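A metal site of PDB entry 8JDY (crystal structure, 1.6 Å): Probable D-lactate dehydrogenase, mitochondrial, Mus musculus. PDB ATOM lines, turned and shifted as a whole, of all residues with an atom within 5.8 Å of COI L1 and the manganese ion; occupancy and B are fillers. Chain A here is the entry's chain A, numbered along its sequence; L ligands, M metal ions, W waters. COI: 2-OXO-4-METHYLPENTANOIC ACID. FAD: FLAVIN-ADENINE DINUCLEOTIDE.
OD2 of Asp 354 is in hydrogen-bond range of N of Glu 429.
The side-chain carboxylate (OE1) of Glu 429 sits close to the backbone NH (N) of Ser 160.
The backbone carbonyl oxygen of His 385 is in hydrogen-bond range of the backbone NH of Asn 390, 3.3 Å away.
OE2 of Glu 264 is in hydrogen-bond range of ND1 of His 385, 2.7 Å away.
The backbone NH of His 392 lies within hydrogen-bond range of the backbone carbonyl oxygen of Val 383 (2.7 Å).
OD1 of Asp 354 sits close to ND1 of His 392.
The backbone NH (N) of His 430 is in hydrogen-bond range of the side-chain carboxylate (OD2) of Asp 354 (2.7 Å).
The side-chain carboxylate (OE1) of Glu 264 is in salt-bridge range of the guanidinium group (NE) of Arg 334, 2.8 Å away.
O3 of COI L1 lies close to NE2 of His 430 (2.7 Å).
The guanidinium group (NH1) of Arg 334 is in salt-bridge range of an oxygen (O1) of COI L1 (3.0 Å).
OE1 of Glu 429 is in hydrogen-bond range of N3 of FAD L2.
N5 of FAD L2 is in hydrogen-bond range of N of Gly 146 (3.1 Å).
N of Ser 160 is in hydrogen-bond range of O2 of FAD L2, at 3.2 Å.
The backbone carbonyl oxygen (O) of Ser 160 lies within hydrogen-bond range of a nitrogen (N3) of FAD L2.
Within 4 Å of the manganese ion: His 385, His 392 and Glu 429.
The nearest printed residue that does not touch the manganese ion is His 430 (4.1 Å).
Residues that only touch COI L1: Trp 338 (3.4 Å) and Ser 352 (3.5 Å).
Hydrophobic or aromatic side chains that line COI L1: Trp 338, His 385, His 392 and His 430.
Within 4 Å of COI L1: Arg 334, Trp 338, Ser 352, His 385, His 392, Glu 429 and His 430.
Water W2 lies within hydrogen-bond range of the backbone NH (N) of Trp 338 (2.8 Å), an oxygen (O1) of COI L1 (2.9 Å), the backbone carbonyl oxygen (O) of His 335 (2.9 Å) and the backbone NH (N) of Ala 337 (3.3 Å).
Water W1 lies within hydrogen-bond range of N of Gly 146 (3.0 Å), O1 of COI L1 (3.2 Å) and NH1 of Arg 334 (3.4 Å).
The manganese ion is bound by OE2 of Glu 429 (2.1 Å), O2 of COI L1 (2.1 Å), NE2 of His 385 (2.3 Å), O3 of COI L1 (2.3 Å) and NE2 of His 392 (2.4 Å).
The manganese ion has five donor atoms within binding distance.
Slightly farther from the manganese ion lies an oxygen (O4) of FAD L2 (2.7 Å).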
ATOM      1  N   VAL A  88      -9.784 -24.448  16.923  1.00  0.00           N
ATOM      2  CA  VAL A  88     -10.372 -25.064  18.112  1.00  0.00           C
ATOM      3  C   VAL A  88      -9.740 -26.409  18.470  1.00  0.00           C
ATOM      4  O   VAL A  88     -10.307 -27.169  19.257  1.00  0.00           O
ATOM      5  CB  VAL A  88     -11.900 -25.210  17.949  1.00  0.00           C
ATOM      6  CG1 VAL A  88     -12.573 -23.845  17.840  1.00  0.00           C
ATOM      7  CG2 VAL A  88     -12.243 -26.051  16.731  1.00  0.00           C
ATOM      8  N   GLY A 146     -17.921 -19.403  11.397  1.00  0.00           N
ATOM      9  CA  GLY A 146     -18.546 -18.371  12.208  1.00  0.00           C
ATOM     10  C   GLY A 146     -17.576 -17.289  12.632  1.00  0.00           C
ATOM     11  O   GLY A 146     -17.980 -16.146  12.857  1.00  0.00           O
ATOM     12  N   SER A 160     -14.727 -25.563   6.524  1.00  0.00           N
ATOM     13  CA  SER A 160     -15.964 -25.465   5.760  1.00  0.00           C
ATOM     14  C   SER A 160     -16.870 -24.465   6.448  1.00  0.00           C
ATOM     15  O   SER A 160     -16.391 -23.560   7.136  1.00  0.00           O
ATOM     16  CB  SER A 160     -16.619 -26.836   5.548  1.00  0.00           C
ATOM     17  OG  SER A 160     -17.255 -27.365   6.698  1.00  0.00           O
ATOM     18  N   GLY A 161     -18.177 -24.608   6.277  1.00  0.00           N
ATOM     19  CA  GLY A 161     -19.092 -23.676   6.916  1.00  0.00           C
ATOM     20  C   GLY A 161     -20.506 -23.969   6.485  1.00  0.00           C
ATOM     21  O   GLY A 161     -20.775 -24.988   5.845  1.00  0.00           O
ATOM     22  N   GLU A 264     -28.858 -25.986   8.471  1.00  0.00           N
ATOM     23  CA  GLU A 264     -28.159 -26.034   9.741  1.00  0.00           C
ATOM     24  C   GLU A 264     -29.108 -26.555  10.815  1.00  0.00           C
ATOM     25  O   GLU A 264     -30.246 -26.096  10.909  1.00  0.00           O
ATOM     26  CB  GLU A 264     -27.669 -24.649  10.136  1.00  0.00           C
ATOM     27  CG  GLU A 264     -26.516 -24.163   9.268  1.00  0.00           C
ATOM     28  CD  GLU A 264     -25.252 -24.966   9.486  1.00  0.00           C
ATOM     29  OE1 GLU A 264     -24.794 -25.083  10.640  1.00  0.00           O
ATOM     30  OE2 GLU A 264     -24.691 -25.465   8.479  1.00  0.00           O
ATOM     31  N   ARG A 334     -26.449 -17.895  14.330  1.00  0.00           N
ATOM     32  CA  ARG A 334     -25.864 -19.206  14.075  1.00  0.00           C
ATOM     33  C   ARG A 334     -24.343 -19.131  14.179  1.00  0.00           C
ATOM     34  O   ARG A 334     -23.712 -19.955  14.848  1.00  0.00           O
ATOM     35  CB  ARG A 334     -26.282 -19.720  12.695  1.00  0.00           C
ATOM     36  CG  ARG A 334     -25.476 -20.904  12.184  1.00  0.00           C
ATOM     37  CD  ARG A 334     -25.614 -22.106  13.095  1.00  0.00           C
ATOM     38  NE  ARG A 334     -24.740 -23.198  12.651  1.00  0.00           N
ATOM     39  CZ  ARG A 334     -23.483 -23.367  13.060  1.00  0.00           C
ATOM     40  NH1 ARG A 334     -22.946 -22.539  13.954  1.00  0.00           N
ATOM     41  NH2 ARG A 334     -22.762 -24.384  12.588  1.00  0.00           N
ATOM     42  N   HIS A 335     -23.743 -18.114  13.539  1.00  0.00           N
ATOM     43  CA  HIS A 335     -22.291 -18.021  13.521  1.00  0.00           C
ATOM     44  C   HIS A 335     -21.711 -17.804  14.907  1.00  0.00           C
ATOM     45  O   HIS A 335     -20.543 -18.127  15.143  1.00  0.00           O
ATOM     46  CB  HIS A 335     -21.862 -16.888  12.580  1.00  0.00           C
ATOM     47  CG  HIS A 335     -21.909 -17.260  11.128  1.00  0.00           C
ATOM     48  ND1 HIS A 335     -22.207 -16.360  10.134  1.00  0.00           N
ATOM     49  CD2 HIS A 335     -21.706 -18.452  10.508  1.00  0.00           C
ATOM     50  CE1 HIS A 335     -22.179 -16.966   8.959  1.00  0.00           C
ATOM     51  NE2 HIS A 335     -21.871 -18.236   9.161  1.00  0.00           N
ATOM     52  N   ALA A 337     -23.005 -19.283  17.651  1.00  0.00           N
ATOM     53  CA  ALA A 337     -23.462 -20.387  18.496  1.00  0.00           C
ATOM     54  C   ALA A 337     -22.413 -20.783  19.540  1.00  0.00           C
ATOM     55  O   ALA A 337     -22.753 -21.123  20.676  1.00  0.00           O
ATOM     56  CB  ALA A 337     -23.816 -21.592  17.629  1.00  0.00           C
ATOM     57  N   TRP A 338     -21.139 -20.775  19.160  1.00  0.00           N
ATOM     58  CA  TRP A 338     -20.065 -21.075  20.114  1.00  0.00           C
ATOM     59  C   TRP A 338     -20.144 -20.184  21.340  1.00  0.00           C
ATOM     60  O   TRP A 338     -20.083 -20.662  22.474  1.00  0.00           O
ATOM     61  CB  TRP A 338     -18.715 -20.873  19.413  1.00  0.00           C
ATOM     62  CG  TRP A 338     -17.471 -21.095  20.239  1.00  0.00           C
ATOM     63  CD1 TRP A 338     -16.563 -20.149  20.607  1.00  0.00           C
ATOM     64  CD2 TRP A 338     -16.951 -22.347  20.720  1.00  0.00           C
ATOM     65  NE1 TRP A 338     -15.529 -20.721  21.301  1.00  0.00           N
ATOM     66  CE2 TRP A 338     -15.738 -22.074  21.386  1.00  0.00           C
ATOM     67  CE3 TRP A 338     -17.402 -23.664  20.663  1.00  0.00           C
ATOM     68  CZ2 TRP A 338     -14.971 -23.065  21.994  1.00  0.00           C
ATOM     69  CZ3 TRP A 338     -16.634 -24.657  21.262  1.00  0.00           C
ATOM     70  CH2 TRP A 338     -15.429 -24.350  21.918  1.00  0.00           C
ATOM     71  N   SER A 352     -15.375 -28.857  21.302  1.00  0.00           N
ATOM     72  CA  SER A 352     -16.320 -29.150  20.236  1.00  0.00           C
ATOM     73  C   SER A 352     -15.876 -30.424  19.515  1.00  0.00           C
ATOM     74  O   SER A 352     -14.690 -30.607  19.223  1.00  0.00           O
ATOM     75  CB  SER A 352     -16.419 -28.013  19.239  1.00  0.00           C
ATOM     76  OG  SER A 352     -17.201 -28.396  18.111  1.00  0.00           O
ATOM     77  N   ASP A 354     -16.692 -32.856  15.988  1.00  0.00           N
ATOM     78  CA  ASP A 354     -16.771 -32.466  14.578  1.00  0.00           C
ATOM     79  C   ASP A 354     -16.875 -33.685  13.661  1.00  0.00           C
ATOM     80  O   ASP A 354     -16.362 -33.666  12.539  1.00  0.00           O
ATOM     81  CB  ASP A 354     -15.550 -31.605  14.225  1.00  0.00           C
ATOM     82  CG  ASP A 354     -15.587 -31.059  12.810  1.00  0.00           C
ATOM     83  OD1 ASP A 354     -16.683 -30.761  12.290  1.00  0.00           O
ATOM     84  OD2 ASP A 354     -14.494 -30.886  12.220  1.00  0.00           O
ATOM     85  N   VAL A 383     -25.130 -28.503  17.276  1.00  0.00           N
ATOM     86  CA  VAL A 383     -25.327 -27.594  16.164  1.00  0.00           C
ATOM     87  C   VAL A 383     -24.501 -28.118  14.997  1.00  0.00           C
ATOM     88  O   VAL A 383     -23.423 -28.704  15.202  1.00  0.00           O
ATOM     89  CB  VAL A 383     -24.913 -26.149  16.550  1.00  0.00           C
ATOM     90  CG1 VAL A 383     -23.403 -26.048  16.803  1.00  0.00           C
ATOM     91  CG2 VAL A 383     -25.345 -25.145  15.495  1.00  0.00           C
ATOM     92  N   GLY A 384     -24.965 -27.900  13.788  1.00  0.00           N
ATOM     93  CA  GLY A 384     -24.014 -27.922  12.691  1.00  0.00           C
ATOM     94  C   GLY A 384     -24.541 -28.316  11.335  1.00  0.00           C
ATOM     95  O   GLY A 384     -25.745 -28.277  11.050  1.00  0.00           O
ATOM     96  N   HIS A 385     -23.570 -28.664  10.482  1.00  0.00           N
ATOM     97  CA  HIS A 385     -23.699 -28.693   9.030  1.00  0.00           C
ATOM     98  C   HIS A 385     -24.217 -30.063   8.596  1.00  0.00           C
ATOM     99  O   HIS A 385     -23.527 -30.857   7.953  1.00  0.00           O
ATOM    100  CB  HIS A 385     -22.360 -28.370   8.394  1.00  0.00           C
ATOM    101  CG  HIS A 385     -21.618 -27.262   9.079  1.00  0.00           C
ATOM    102  ND1 HIS A 385     -22.109 -25.979   9.161  1.00  0.00           N
ATOM    103  CD2 HIS A 385     -20.401 -27.245   9.699  1.00  0.00           C
ATOM    104  CE1 HIS A 385     -21.236 -25.225   9.817  1.00  0.00           C
ATOM    105  NE2 HIS A 385     -20.205 -25.967  10.162  1.00  0.00           N
ATOM    106  N   ASN A 390     -22.480 -33.787   8.971  1.00  0.00           N
ATOM    107  CA  ASN A 390     -21.515 -33.260   9.927  1.00  0.00           C
ATOM    108  C   ASN A 390     -22.277 -32.552  11.044  1.00  0.00           C
ATOM    109  O   ASN A 390     -23.331 -31.959  10.801  1.00  0.00           O
ATOM    110  CB  ASN A 390     -20.566 -32.310   9.132  1.00  0.00           C
ATOM    111  CG  ASN A 390     -19.554 -31.556   9.994  1.00  0.00           C
ATOM    112  OD1 ASN A 390     -19.394 -30.340   9.805  1.00  0.00           O
ATOM    113  ND2 ASN A 390     -18.802 -32.245  10.856  1.00  0.00           N
ATOM    114  N   HIS A 392     -21.587 -30.674  15.307  1.00  0.00           N
ATOM    115  CA  HIS A 392     -20.740 -30.325  16.436  1.00  0.00           C
ATOM    116  C   HIS A 392     -21.503 -30.572  17.715  1.00  0.00           C
ATOM    117  O   HIS A 392     -22.659 -30.146  17.834  1.00  0.00           O
ATOM    118  CB  HIS A 392     -20.333 -28.854  16.407  1.00  0.00           C
ATOM    119  CG  HIS A 392     -19.738 -28.407  15.111  1.00  0.00           C
ATOM    120  ND1 HIS A 392     -18.568 -28.931  14.589  1.00  0.00           N
ATOM    121  CD2 HIS A 392     -20.140 -27.462  14.231  1.00  0.00           C
ATOM    122  CE1 HIS A 392     -18.296 -28.341  13.445  1.00  0.00           C
ATOM    123  NE2 HIS A 392     -19.224 -27.428  13.208  1.00  0.00           N
ATOM    124  N   ILE A 394     -21.085 -29.322  21.427  1.00  0.00           N
ATOM    125  CA  ILE A 394     -20.361 -28.323  22.206  1.00  0.00           C
ATOM    126  C   ILE A 394     -20.506 -28.686  23.669  1.00  0.00           C
ATOM    127  O   ILE A 394     -21.598 -28.571  24.247  1.00  0.00           O
ATOM    128  CB  ILE A 394     -20.898 -26.902  21.945  1.00  0.00           C
ATOM    129  CG1 ILE A 394     -20.742 -26.511  20.478  1.00  0.00           C
ATOM    130  CG2 ILE A 394     -20.202 -25.883  22.850  1.00  0.00           C
ATOM    131  CD1 ILE A 394     -21.341 -25.162  20.158  1.00  0.00           C
ATOM    132  N   GLU A 429     -14.163 -30.676   9.471  1.00  0.00           N
ATOM    133  CA  GLU A 429     -13.646 -29.363   9.092  1.00  0.00           C
ATOM    134  C   GLU A 429     -12.633 -28.742  10.068  1.00  0.00           C
ATOM    135  O   GLU A 429     -11.771 -27.974   9.642  1.00  0.00           O
ATOM    136  CB  GLU A 429     -14.802 -28.393   8.880  1.00  0.00           C
ATOM    137  CG  GLU A 429     -15.685 -28.265  10.135  1.00  0.00           C
ATOM    138  CD  GLU A 429     -16.687 -27.152  10.046  1.00  0.00           C
ATOM    139  OE1 GLU A 429     -16.925 -26.626   8.939  1.00  0.00           O
ATOM    140  OE2 GLU A 429     -17.218 -26.773  11.117  1.00  0.00           O
ATOM    141  N   HIS A 430     -12.740 -29.025  11.374  1.00  0.00           N
ATOM    142  CA  HIS A 430     -11.916 -28.312  12.353  1.00  0.00           C
ATOM    143  C   HIS A 430     -10.456 -28.743  12.308  1.00  0.00           C
ATOM    144  O   HIS A 430      -9.567 -27.966  12.659  1.00  0.00           O
ATOM    145  CB  HIS A 430     -12.422 -28.547  13.776  1.00  0.00           C
ATOM    146  CG  HIS A 430     -13.695 -27.837  14.068  1.00  0.00           C
ATOM    147  ND1 HIS A 430     -14.504 -28.175  15.129  1.00  0.00           N
ATOM    148  CD2 HIS A 430     -14.302 -26.798  13.450  1.00  0.00           C
ATOM    149  CE1 HIS A 430     -15.552 -27.372  15.154  1.00  0.00           C
ATOM    150  NE2 HIS A 430     -15.460 -26.522  14.146  1.00  0.00           N
HETATM  151  C1  COI L   1     -19.608 -23.986  14.018  1.00  0.00           C
HETATM  152  O1  COI L   1     -20.154 -23.095  14.730  1.00  0.00           O
HETATM  153  O2  COI L   1     -20.089 -24.328  12.910  1.00  0.00           O
HETATM  154  C2  COI L   1     -18.351 -24.689  14.462  1.00  0.00           C
HETATM  155  O3  COI L   1     -17.518 -24.926  13.651  1.00  0.00           O
HETATM  156  C3  COI L   1     -18.198 -25.078  15.919  1.00  0.00           C
HETATM  157  C4  COI L   1     -17.072 -24.220  16.456  1.00  0.00           C
HETATM  158  C5  COI L   1     -17.661 -22.884  16.872  1.00  0.00           C
HETATM  159  C6  COI L   1     -16.468 -24.913  17.654  1.00  0.00           C
HETATM  160  PA  FAD L   2      -5.251 -20.399  13.767  1.00  0.00           P
HETATM  161  O1A FAD L   2      -5.895 -20.821  15.037  1.00  0.00           O
HETATM  162  O2A FAD L   2      -4.409 -19.160  13.702  1.00  0.00           O
HETATM  163  O5B FAD L   2      -4.404 -21.619  13.190  1.00  0.00           O
HETATM  164  C5B FAD L   2      -5.038 -22.904  12.963  1.00  0.00           C
HETATM  165  C4B FAD L   2      -4.015 -23.906  12.477  1.00  0.00           C
HETATM  166  O4B FAD L   2      -3.616 -23.566  11.133  1.00  0.00           O
HETATM  167  C3B FAD L   2      -2.732 -23.981  13.298  1.00  0.00           C
HETATM  168  O3B FAD L   2      -2.261 -25.318  13.307  1.00  0.00           O
HETATM  169  C2B FAD L   2      -1.823 -22.995  12.571  1.00  0.00           C
HETATM  170  O2B FAD L   2      -0.437 -23.268  12.747  1.00  0.00           O
HETATM  171  C1B FAD L   2      -2.248 -23.193  11.119  1.00  0.00           C
HETATM  172  N9A FAD L   2      -2.137 -22.013  10.280  1.00  0.00           N
HETATM  173  C8A FAD L   2      -2.797 -20.813  10.399  1.00  0.00           C
HETATM  174  N7A FAD L   2      -2.510 -19.952   9.448  1.00  0.00           N
HETATM  175  C5A FAD L   2      -1.630 -20.650   8.624  1.00  0.00           C
HETATM  176  C6A FAD L   2      -0.968 -20.296   7.446  1.00  0.00           C
HETATM  177  N6A FAD L   2      -1.098 -19.121   6.842  1.00  0.00           N
HETATM  178  N1A FAD L   2      -0.141 -21.225   6.893  1.00  0.00           N
HETATM  179  C2A FAD L   2      -0.022 -22.409   7.487  1.00  0.00           C
HETATM  180  N3A FAD L   2      -0.610 -22.852   8.606  1.00  0.00           N
HETATM  181  C4A FAD L   2      -1.406 -21.918   9.133  1.00  0.00           C
HETATM  182  N1  FAD L   2     -14.014 -23.784  11.410  1.00  0.00           N
HETATM  183  C2  FAD L   2     -14.647 -24.374  10.359  1.00  0.00           C
HETATM  184  O2  FAD L   2     -14.027 -25.111   9.564  1.00  0.00           O
HETATM  185  N3  FAD L   2     -15.991 -24.130  10.156  1.00  0.00           N
HETATM  186  C4  FAD L   2     -16.809 -23.342  10.941  1.00  0.00           C
HETATM  187  O4  FAD L   2     -18.006 -23.227  10.682  1.00  0.00           O
HETATM  188  C4X FAD L   2     -16.120 -22.702  12.045  1.00  0.00           C
HETATM  189  N5  FAD L   2     -16.818 -21.903  12.842  1.00  0.00           N
HETATM  190  C5X FAD L   2     -16.150 -21.304  13.898  1.00  0.00           C
HETATM  191  C6  FAD L   2     -16.868 -20.459  14.743  1.00  0.00           C
HETATM  192  C7  FAD L   2     -16.254 -19.836  15.824  1.00  0.00           C
HETATM  193  C7M FAD L   2     -17.057 -18.940  16.724  1.00  0.00           C
HETATM  194  C8  FAD L   2     -14.892 -20.058  16.068  1.00  0.00           C
HETATM  195  C8M FAD L   2     -14.187 -19.394  17.221  1.00  0.00           C
HETATM  196  C9  FAD L   2     -14.171 -20.894  15.221  1.00  0.00           C
HETATM  197  C9A FAD L   2     -14.785 -21.517  14.140  1.00  0.00           C
HETATM  198  N10 FAD L   2     -14.074 -22.356  13.250  1.00  0.00           N
HETATM  199  C10 FAD L   2     -14.718 -22.973  12.203  1.00  0.00           C
HETATM  200  C1' FAD L   2     -12.657 -22.693  13.509  1.00  0.00           C
HETATM  201  C2' FAD L   2     -11.646 -21.727  12.902  1.00  0.00           C
HETATM  202  O2' FAD L   2     -12.244 -20.448  12.692  1.00  0.00           O
HETATM  203  C3' FAD L   2     -11.123 -22.300  11.591  1.00  0.00           C
HETATM  204  O3' FAD L   2     -10.459 -23.525  11.897  1.00  0.00           O
HETATM  205  C4' FAD L   2     -10.159 -21.365  10.876  1.00  0.00           C
HETATM  206  O4' FAD L   2      -9.845 -21.922   9.592  1.00  0.00           O
HETATM  207  C5' FAD L   2      -8.893 -21.125  11.665  1.00  0.00           C
HETATM  208  O5' FAD L   2      -8.169 -20.030  11.064  1.00  0.00           O
HETATM  209  P   FAD L   2      -7.163 -19.167  11.921  1.00  0.00           P
HETATM  210  O1P FAD L   2      -6.246 -18.313  11.048  1.00  0.00           O
HETATM  211  O2P FAD L   2      -7.902 -18.379  12.973  1.00  0.00           O
HETATM  212  O3P FAD L   2      -6.334 -20.331  12.612  1.00  0.00           O
HETATM  213 MN    MN M   1     -18.739 -25.574  11.824  1.00  0.00          MN
HETATM  214  O   HOH W   1     -20.306 -20.935  12.437  1.00  0.00           O
HETATM  215  O   HOH W   2     -20.269 -20.749  16.447  1.00  0.00           O
